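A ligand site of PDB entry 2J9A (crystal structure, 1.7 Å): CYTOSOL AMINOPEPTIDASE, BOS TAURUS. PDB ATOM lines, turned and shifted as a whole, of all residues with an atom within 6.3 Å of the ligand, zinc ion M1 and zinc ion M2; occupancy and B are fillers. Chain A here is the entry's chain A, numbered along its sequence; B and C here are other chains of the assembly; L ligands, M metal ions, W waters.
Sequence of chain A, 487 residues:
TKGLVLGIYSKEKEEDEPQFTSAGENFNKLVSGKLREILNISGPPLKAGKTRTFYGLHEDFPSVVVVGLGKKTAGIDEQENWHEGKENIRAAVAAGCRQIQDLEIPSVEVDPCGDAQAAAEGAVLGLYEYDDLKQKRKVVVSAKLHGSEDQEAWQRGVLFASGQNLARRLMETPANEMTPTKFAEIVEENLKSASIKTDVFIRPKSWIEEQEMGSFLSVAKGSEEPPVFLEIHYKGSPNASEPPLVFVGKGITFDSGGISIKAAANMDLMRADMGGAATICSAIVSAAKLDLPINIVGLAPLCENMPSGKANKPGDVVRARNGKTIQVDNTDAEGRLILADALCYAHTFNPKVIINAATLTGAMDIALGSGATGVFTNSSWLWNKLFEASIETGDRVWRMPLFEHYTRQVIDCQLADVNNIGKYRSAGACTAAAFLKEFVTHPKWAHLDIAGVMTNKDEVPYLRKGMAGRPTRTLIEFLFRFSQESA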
ATOM      1  N   LYS A 250      13.526  30.152 -12.895  1.00  0.00           N
ATOM      2  CA  LYS A 250      12.960  30.666 -11.656  1.00  0.00           C
ATOM      3  C   LYS A 250      13.766  30.171 -10.426  1.00  0.00           C
ATOM      4  O   LYS A 250      13.908  28.960 -10.247  1.00  0.00           O
ATOM      5  CB  LYS A 250      11.487  30.210 -11.567  1.00  0.00           C
ATOM      6  CG  LYS A 250      10.835  30.443 -10.177  1.00  0.00           C
ATOM      7  CD  LYS A 250       9.359  29.834 -10.196  1.00  0.00           C
ATOM      8  CE  LYS A 250       8.778  29.922  -8.777  1.00  0.00           C
ATOM      9  NZ  LYS A 250       7.478  29.184  -8.662  1.00  0.00           N
ATOM     10  N   ILE A 252      13.257  30.617  -6.950  1.00  0.00           N
ATOM     11  CA  ILE A 252      12.692  30.895  -5.630  1.00  0.00           C
ATOM     12  C   ILE A 252      13.270  29.843  -4.652  1.00  0.00           C
ATOM     13  O   ILE A 252      12.931  28.653  -4.720  1.00  0.00           O
ATOM     14  CB  ILE A 252      11.150  30.801  -5.701  1.00  0.00           C
ATOM     15  CG1 ILE A 252      10.622  31.987  -6.538  1.00  0.00           C
ATOM     16  CG2 ILE A 252      10.560  30.813  -4.262  1.00  0.00           C
ATOM     17  CD1 ILE A 252      10.901  33.401  -5.889  1.00  0.00           C
ATOM     18  N   ASP A 255       9.458  28.874  -1.277  1.00  0.00           N
ATOM     19  CA  ASP A 255       8.145  29.531  -1.548  1.00  0.00           C
ATOM     20  C   ASP A 255       7.135  29.175  -0.424  1.00  0.00           C
ATOM     21  O   ASP A 255       6.575  28.073  -0.376  1.00  0.00           O
ATOM     22  CB  ASP A 255       7.588  29.071  -2.901  1.00  0.00           C
ATOM     23  CG  ASP A 255       6.346  29.853  -3.327  1.00  0.00           C
ATOM     24  OD1 ASP A 255       6.051  30.866  -2.667  1.00  0.00           O
ATOM     25  OD2 ASP A 255       5.734  29.441  -4.329  1.00  0.00           O
ATOM     26  N   SER A 256       6.922  30.136   0.493  1.00  0.00           N
ATOM     27  CA  SER A 256       5.876  29.985   1.517  1.00  0.00           C
ATOM     28  C   SER A 256       4.507  30.406   0.945  1.00  0.00           C
ATOM     29  O   SER A 256       3.472  30.265   1.646  1.00  0.00           O
ATOM     30  CB  SER A 256       6.163  30.878   2.750  1.00  0.00           C
ATOM     31  OG  SER A 256       6.020  32.257   2.359  1.00  0.00           O
ATOM     32  N   GLY A 257       4.519  30.943  -0.263  1.00  0.00           N
ATOM     33  CA  GLY A 257       3.352  31.672  -0.814  1.00  0.00           C
ATOM     34  C   GLY A 257       3.325  33.165  -0.503  1.00  0.00           C
ATOM     35  O   GLY A 257       2.642  33.935  -1.207  1.00  0.00           O
ATOM     36  N   LYS A 262       0.752  29.477   1.742  1.00  0.00           N
ATOM     37  CA  LYS A 262       0.409  28.063   1.436  1.00  0.00           C
ATOM     38  C   LYS A 262      -0.039  27.333   2.698  1.00  0.00           C
ATOM     39  O   LYS A 262       0.300  27.738   3.800  1.00  0.00           O
ATOM     40  CB  LYS A 262       1.661  27.339   0.901  1.00  0.00           C
ATOM     41  CG  LYS A 262       2.018  27.831  -0.523  1.00  0.00           C
ATOM     42  CD  LYS A 262       3.301  27.158  -0.988  1.00  0.00           C
ATOM     43  CE  LYS A 262       3.701  27.561  -2.447  1.00  0.00           C
ATOM     44  NZ  LYS A 262       2.556  27.332  -3.447  1.00  0.00           N
ATOM     45  N   LEU A 269       8.454  20.809   0.388  1.00  0.00           N
ATOM     46  CA  LEU A 269       8.920  20.567  -1.020  1.00  0.00           C
ATOM     47  C   LEU A 269       9.223  21.881  -1.746  1.00  0.00           C
ATOM     48  O   LEU A 269       9.913  21.862  -2.796  1.00  0.00           O
ATOM     49  CB  LEU A 269       7.863  19.812  -1.817  1.00  0.00           C
ATOM     50  CG  LEU A 269       7.630  18.386  -1.253  1.00  0.00           C
ATOM     51  CD1 LEU A 269       6.469  17.766  -2.079  1.00  0.00           C
ATOM     52  CD2 LEU A 269       8.895  17.505  -1.302  1.00  0.00           C
ATOM     53  N   MET A 270       8.733  22.993  -1.200  1.00  0.00           N
ATOM     54  CA  MET A 270       8.961  24.300  -1.824  1.00  0.00           C
ATOM     55  C   MET A 270      10.415  24.772  -1.695  1.00  0.00           C
ATOM     56  O   MET A 270      10.776  25.804  -2.268  1.00  0.00           O
ATOM     57  CB  MET A 270       7.992  25.375  -1.298  1.00  0.00           C
ATOM     58  CG  MET A 270       6.497  25.106  -1.703  1.00  0.00           C
ATOM     59  SD  MET A 270       6.301  25.004  -3.534  1.00  0.00           S
ATOM     60  CE  MET A 270       6.472  23.249  -3.877  1.00  0.00           C
ATOM     61  N   ASP A 273      11.691  25.110  -5.209  1.00  0.00           N
ATOM     62  CA  ASP A 273      11.077  26.111  -6.095  1.00  0.00           C
ATOM     63  C   ASP A 273      12.130  26.905  -6.847  1.00  0.00           C
ATOM     64  O   ASP A 273      11.776  27.825  -7.564  1.00  0.00           O
ATOM     65  CB  ASP A 273      10.179  27.049  -5.313  1.00  0.00           C
ATOM     66  CG  ASP A 273       9.031  27.596  -6.165  1.00  0.00           C
ATOM     67  OD1 ASP A 273       8.667  26.966  -7.176  1.00  0.00           O
ATOM     68  OD2 ASP A 273       8.531  28.647  -5.743  1.00  0.00           O
ATOM     69  N   ASN A 305      10.312  33.723  -0.980  1.00  0.00           N
ATOM     70  CA  ASN A 305       8.955  34.312  -0.976  1.00  0.00           C
ATOM     71  C   ASN A 305       8.373  34.089   0.415  1.00  0.00           C
ATOM     72  O   ASN A 305       7.912  32.974   0.722  1.00  0.00           O
ATOM     73  CB  ASN A 305       8.047  33.684  -2.082  1.00  0.00           C
ATOM     74  CG  ASN A 305       6.722  34.453  -2.256  1.00  0.00           C
ATOM     75  OD1 ASN A 305       6.650  35.675  -1.986  1.00  0.00           O
ATOM     76  ND2 ASN A 305       5.690  33.765  -2.761  1.00  0.00           N
ATOM     77  N   THR A 331       0.008  36.543  -4.082  1.00  0.00           N
ATOM     78  CA  THR A 331       1.474  36.669  -3.873  1.00  0.00           C
ATOM     79  C   THR A 331       2.188  35.328  -4.056  1.00  0.00           C
ATOM     80  O   THR A 331       3.441  35.295  -4.047  1.00  0.00           O
ATOM     81  CB  THR A 331       1.837  37.222  -2.470  1.00  0.00           C
ATOM     82  OG1 THR A 331       1.454  36.264  -1.450  1.00  0.00           O
ATOM     83  CG2 THR A 331       1.157  38.574  -2.199  1.00  0.00           C
ATOM     84  N   ASP A 332       1.426  34.251  -4.221  1.00  0.00           N
ATOM     85  CA  ASP A 332       2.004  32.921  -4.427  1.00  0.00           C
ATOM     86  C   ASP A 332       2.166  32.616  -5.933  1.00  0.00           C
ATOM     87  O   ASP A 332       2.703  31.585  -6.310  1.00  0.00           O
ATOM     88  CB  ASP A 332       1.103  31.872  -3.760  1.00  0.00           C
ATOM     89  CG  ASP A 332       1.737  30.489  -3.610  1.00  0.00           C
ATOM     90  OD1 ASP A 332       2.970  30.285  -3.842  1.00  0.00           O
ATOM     91  OD2 ASP A 332       0.948  29.575  -3.235  1.00  0.00           O
ATOM     92  N   ALA A 333       1.717  33.560  -6.767  1.00  0.00           N
ATOM     93  CA  ALA A 333       2.037  33.504  -8.196  1.00  0.00           C
ATOM     94  C   ALA A 333       3.301  34.382  -8.411  1.00  0.00           C
ATOM     95  O   ALA A 333       3.306  35.326  -9.208  1.00  0.00           O
ATOM     96  CB  ALA A 333       0.836  34.008  -9.062  1.00  0.00           C
ATOM     97  N   GLU A 334       4.340  34.074  -7.640  1.00  0.00           N
ATOM     98  CA  GLU A 334       5.539  34.915  -7.592  1.00  0.00           C
ATOM     99  C   GLU A 334       6.531  34.543  -8.686  1.00  0.00           C
ATOM    100  O   GLU A 334       7.320  35.404  -9.096  1.00  0.00           O
ATOM    101  CB  GLU A 334       6.220  34.828  -6.204  1.00  0.00           C
ATOM    102  CG  GLU A 334       7.189  33.584  -6.009  1.00  0.00           C
ATOM    103  CD  GLU A 334       6.457  32.213  -5.974  1.00  0.00           C
ATOM    104  OE1 GLU A 334       5.273  32.189  -5.568  1.00  0.00           O
ATOM    105  OE2 GLU A 334       7.067  31.189  -6.302  1.00  0.00           O
ATOM    106  N   GLY A 335       6.521  33.302  -9.138  1.00  0.00           N
ATOM    107  CA  GLY A 335       7.460  32.896 -10.225  1.00  0.00           C
ATOM    108  C   GLY A 335       7.284  33.723 -11.476  1.00  0.00           C
ATOM    109  O   GLY A 335       8.268  34.170 -12.136  1.00  0.00           O
ATOM    110  N   THR A 359       9.346  25.866 -11.808  1.00  0.00           N
ATOM    111  CA  THR A 359       8.388  25.007 -11.063  1.00  0.00           C
ATOM    112  C   THR A 359       7.128  25.889 -10.838  1.00  0.00           C
ATOM    113  O   THR A 359       6.897  26.381  -9.746  1.00  0.00           O
ATOM    114  CB  THR A 359       9.022  24.562  -9.735  1.00  0.00           C
ATOM    115  OG1 THR A 359       9.681  25.695  -9.153  1.00  0.00           O
ATOM    116  CG2 THR A 359      10.074  23.417  -9.957  1.00  0.00           C
ATOM    117  N   LEU A 360       6.376  26.169 -11.905  1.00  0.00           N
ATOM    118  CA  LEU A 360       5.588  27.403 -11.908  1.00  0.00           C
ATOM    119  C   LEU A 360       4.174  27.260 -11.312  1.00  0.00           C
ATOM    120  O   LEU A 360       3.686  28.184 -10.693  1.00  0.00           O
ATOM    121  CB  LEU A 360       5.515  28.018 -13.335  1.00  0.00           C
ATOM    122  CG  LEU A 360       5.153  29.520 -13.386  1.00  0.00           C
ATOM    123  CD1 LEU A 360       6.179  30.402 -12.664  1.00  0.00           C
ATOM    124  CD2 LEU A 360       4.939  29.986 -14.867  1.00  0.00           C
ATOM    125  N   THR A 361       3.508  26.146 -11.629  1.00  0.00           N
ATOM    126  CA  THR A 361       2.105  26.074 -11.246  1.00  0.00           C
ATOM    127  C   THR A 361       1.717  24.733 -10.712  1.00  0.00           C
ATOM    128  O   THR A 361       2.161  23.712 -11.215  1.00  0.00           O
ATOM    129  CB  THR A 361       1.157  26.434 -12.468  1.00  0.00           C
ATOM    130  OG1 THR A 361       1.267  25.462 -13.511  1.00  0.00           O
ATOM    131  CG2 THR A 361       1.465  27.830 -13.074  1.00  0.00           C
ATOM    132  N   GLY A 362       0.816  24.722  -9.719  1.00  0.00           N
ATOM    133  CA  GLY A 362       0.197  23.471  -9.289  1.00  0.00           C
ATOM    134  C   GLY A 362      -0.618  22.899 -10.422  1.00  0.00           C
ATOM    135  O   GLY A 362      -0.733  21.647 -10.544  1.00  0.00           O
ATOM    136  N   ALA A 363      -1.144  23.767 -11.275  1.00  0.00           N
ATOM    137  CA  ALA A 363      -2.003  23.319 -12.378  1.00  0.00           C
ATOM    138  C   ALA A 363      -1.244  22.400 -13.337  1.00  0.00           C
ATOM    139  O   ALA A 363      -1.795  21.433 -13.892  1.00  0.00           O
ATOM    140  CB  ALA A 363      -2.554  24.509 -13.139  1.00  0.00           C
ATOM    141  N   ASP A 365       1.053  20.222 -12.518  1.00  0.00           N
ATOM    142  CA  ASP A 365       1.073  18.905 -11.903  1.00  0.00           C
ATOM    143  C   ASP A 365      -0.288  18.221 -12.072  1.00  0.00           C
ATOM    144  O   ASP A 365      -0.380  17.040 -12.401  1.00  0.00           O
ATOM    145  CB  ASP A 365       1.381  19.009 -10.398  1.00  0.00           C
ATOM    146  CG  ASP A 365       1.449  17.649  -9.779  1.00  0.00           C
ATOM    147  OD1 ASP A 365       2.289  16.858 -10.248  1.00  0.00           O
ATOM    148  OD2 ASP A 365       0.558  17.322  -8.993  1.00  0.00           O
ATOM    149  N   ALA A 451       6.857  22.045 -12.702  1.00  0.00           N
ATOM    150  CA  ALA A 451       6.279  21.758 -11.376  1.00  0.00           C
ATOM    151  C   ALA A 451       5.902  20.280 -11.206  1.00  0.00           C
ATOM    152  O   ALA A 451       6.081  19.695 -10.122  1.00  0.00           O
ATOM    153  CB  ALA A 451       5.015  22.660 -11.101  1.00  0.00           C
ATOM    154  N   GLY A 452       5.379  19.648 -12.259  1.00  0.00           N
ATOM    155  CA  GLY A 452       4.977  18.234 -12.142  1.00  0.00           C
ATOM    156  C   GLY A 452       6.146  17.232 -12.102  1.00  0.00           C
ATOM    157  O   GLY A 452       5.999  16.139 -11.598  1.00  0.00           O
ATOM    158  N   MET A 454       9.067  17.975 -10.624  1.00  0.00           N
ATOM    159  CA  MET A 454       9.967  18.428  -9.547  1.00  0.00           C
ATOM    160  C   MET A 454      10.474  17.270  -8.668  1.00  0.00           C
ATOM    161  O   MET A 454      11.638  17.285  -8.224  1.00  0.00           O
ATOM    162  CB  MET A 454       9.229  19.459  -8.663  1.00  0.00           C
ATOM    163  CG  MET A 454      10.106  20.472  -7.933  1.00  0.00           C
ATOM    164  SD  MET A 454       9.055  21.602  -6.970  1.00  0.00           S
ATOM    165  CE  MET A 454       8.287  20.395  -5.867  1.00  0.00           C
ATOM    166  N   THR A 455       9.605  16.300  -8.414  1.00  0.00           N
ATOM    167  CA  THR A 455       9.943  15.169  -7.529  1.00  0.00           C
ATOM    168  C   THR A 455       9.767  13.832  -8.259  1.00  0.00           C
ATOM    169  O   THR A 455       9.110  13.753  -9.319  1.00  0.00           O
ATOM    170  CB  THR A 455       9.020  15.129  -6.268  1.00  0.00           C
ATOM    171  OG1 THR A 455       7.687  14.782  -6.695  1.00  0.00           O
ATOM    172  CG2 THR A 455       8.985  16.473  -5.568  1.00  0.00           C
ATOM    173  N   ALA B   1       1.955  28.999  -8.330  1.00  0.00           N
ATOM    174  CA  ALA B   1       0.575  29.453  -8.270  1.00  0.00           C
ATOM    175  C   ALA B   1      -0.355  28.287  -7.977  1.00  0.00           C
ATOM    176  O   ALA B   1      -0.175  27.232  -8.577  1.00  0.00           O
ATOM    177  CB  ALA B   1       0.154  30.123  -9.604  1.00  0.00           C
ATOM    178  N   MLE B   2      -1.340  28.523  -7.087  1.00  0.00           N
ATOM    179  CN  MLE B   2      -1.442  29.862  -6.467  1.00  0.00           C
ATOM    180  CA  MLE B   2      -2.306  27.414  -6.784  1.00  0.00           C
ATOM    181  CB  MLE B   2      -2.382  27.152  -5.285  1.00  0.00           C
ATOM    182  CG  MLE B   2      -0.970  26.727  -4.762  1.00  0.00           C
ATOM    183  CD1 MLE B   2      -1.046  26.356  -3.278  1.00  0.00           C
ATOM    184  CD2 MLE B   2      -0.346  25.558  -5.539  1.00  0.00           C
ATOM    185  C   MLE B   2      -3.645  27.673  -7.568  1.00  0.00           C
ATOM    186  O   MLE B   2      -3.809  28.756  -8.159  1.00  0.00           O
ATOM    187  N   ARG C 425      -3.024  12.559  -6.836  1.00  0.00           N
ATOM    188  CA  ARG C 425      -3.850  13.592  -7.420  1.00  0.00           C
ATOM    189  C   ARG C 425      -3.356  14.046  -8.795  1.00  0.00           C
ATOM    190  O   ARG C 425      -4.117  14.550  -9.629  1.00  0.00           O
ATOM    191  CB  ARG C 425      -3.997  14.824  -6.497  1.00  0.00           C
ATOM    192  CG  ARG C 425      -2.642  15.474  -6.098  1.00  0.00           C
ATOM    193  CD  ARG C 425      -2.595  17.022  -6.288  1.00  0.00           C
ATOM    194  NE  ARG C 425      -1.201  17.488  -6.464  1.00  0.00           N
ATOM    195  CZ  ARG C 425      -0.813  18.750  -6.703  1.00  0.00           C
ATOM    196  NH1 ARG C 425       0.479  19.021  -6.835  1.00  0.00           N
ATOM    197  NH2 ARG C 425      -1.683  19.743  -6.798  1.00  0.00           N
ATOM    198  N   SER C 426      -2.094  13.775  -9.081  1.00  0.00           N
ATOM    199  CA  SER C 426      -1.474  14.386 -10.268  1.00  0.00           C
ATOM    200  C   SER C 426      -2.007  13.757 -11.542  1.00  0.00           C
ATOM    201  O   SER C 426      -2.277  12.567 -11.571  1.00  0.00           O
ATOM    202  CB  SER C 426       0.025  14.119 -10.213  1.00  0.00           C
ATOM    203  OG  SER C 426       0.518  14.629  -8.969  1.00  0.00           O
HETATM  204  C1  LIG L   1       4.277  18.957  -5.917  1.00  0.00           C
HETATM  205  C2  LIG L   1       4.057  19.494  -7.347  1.00  0.00           C
HETATM  206  C3  LIG L   1       3.256  20.826  -7.403  1.00  0.00           C
HETATM  207  C4  LIG L   1       4.045  22.005  -6.809  1.00  0.00           C
HETATM  208  C5  LIG L   1       3.524  23.343  -7.396  1.00  0.00           C
HETATM  209  C6  LIG L   1       4.325  24.527  -6.810  1.00  0.00           C
HETATM  210  C7  LIG L   1       3.963  25.832  -7.492  1.00  0.00           C
HETATM  211  C8  LIG L   1       4.524  27.055  -6.724  1.00  0.00           C
HETATM  212  N1  LIG L   1       6.033  27.065  -6.762  1.00  0.00           N
HETATM  213  C9  LIG L   1       4.065  28.329  -7.439  1.00  0.00           C
HETATM  214  O1  LIG L   1       4.669  29.474  -6.891  1.00  0.00           O
HETATM  215  C10 LIG L   1       2.578  28.612  -7.243  1.00  0.00           C
HETATM  216  O2  LIG L   1       2.074  28.479  -6.128  1.00  0.00           O
HETATM  217 ZN    ZN M   1       4.261  30.476  -5.265  1.00  0.00          ZN
HETATM  218 ZN    ZN M   2       6.778  29.125  -6.638  1.00  0.00          ZN
HETATM  219  O   HOH W   1       5.107  30.979  -9.017  1.00  0.00           O
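An oxygen (O2) of the ligand sits at hydrogen-bond distance from the side-chain amino group (NZ) of Lys 262 (3.0 Å). O of Thr 359 lies close to N1 of the ligand, 3.2 Å away. A carbon (C10) of the ligand is covalently linked to the backbone NH (N) of Ala 1 of chain B (1.3 Å).
O of Leu 360 lies within hydrogen-bond range of N of Ala 1 of chain B (3.0 Å). N of Asp 255 is in hydrogen-bond range of O of Met 270, 3.5 Å away. The side-chain carboxylate (OD2) of Asp 332 lies within salt-bridge range of the side-chain amino group (NZ) of Lys 262. The side-chain carboxylate of Asp 255 sits at hydrogen-bond distance from the side-chain amide nitrogen of Asn 305. The side-chain hydroxyl of Ser 426 of chain C is in hydrogen-bond range of the side-chain carboxylate of Asp 365 (2.7 Å). The backbone NH of Gly 257 lies within hydrogen-bond range of the side-chain carboxylate of Asp 255, at 2.9 Å. N of Asp 332 sits at hydrogen-bond distance from O of Gly 257, at 3.3 Å. The backbone carbonyl oxygen of Ser 256 lies within hydrogen-bond range of the backbone NH of Lys 262 (2.8 Å).
Residues that only touch the ligand: Leu 360 (3.3 Å), Arg 425 of chain C (3.4 Å), Ala 451 (3.4 Å), MLE 2 of chain B (3.5 Å), Gly 362 (3.8 Å), Met 270 (3.8 Å) and Asp 365 (3.97 Å). Hydrophobic or aromatic side chains that line the ligand: Met 270 and Ala 1 of chain B. 15 residues have an atom within 4 Å of the ligand: Lys 250, Asp 255, Lys 262, Met 270, Asp 273, Asp 332, Glu 334, Thr 359, Leu 360, Gly 362, Asp 365, Ala 451, Ala 1 of chain B, MLE 2 of chain B and Arg 425 of chain C. Along chain A the residues within 4 Å of the ligand span positions 250 to 451. The nearest printed residue that does not touch the ligand is Thr 361 (4.02 Å).
Of the 29 residues printed, 3 come within 4 Å of zinc ion M1.
The nearest printed residue that does not touch zinc ion M2 is Thr 359 (4.1 Å).
Zinc ion M1 is bound by the side-chain carboxylate of Asp 332 (1.9 Å), an oxygen (O1) of the ligand (2.0 Å), the side-chain carboxylate of Glu 334 (2.0 Å), the side-chain carboxylate of Asp 255 (2.0 Å) and the backbone carbonyl oxygen of Asp 332 (2.2 Å). Zinc ion M1 has five donor atoms within binding distance.
Zinc ion M2 is bound by OD2 of Asp 273 (2.0 Å), OE2 of Glu 334 (2.1 Å), NZ of Lys 250 (2.1 Å), O1 of the ligand (2.2 Å), N1 of the ligand (2.2 Å) and OD2 of Asp 255 (2.6 Å).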
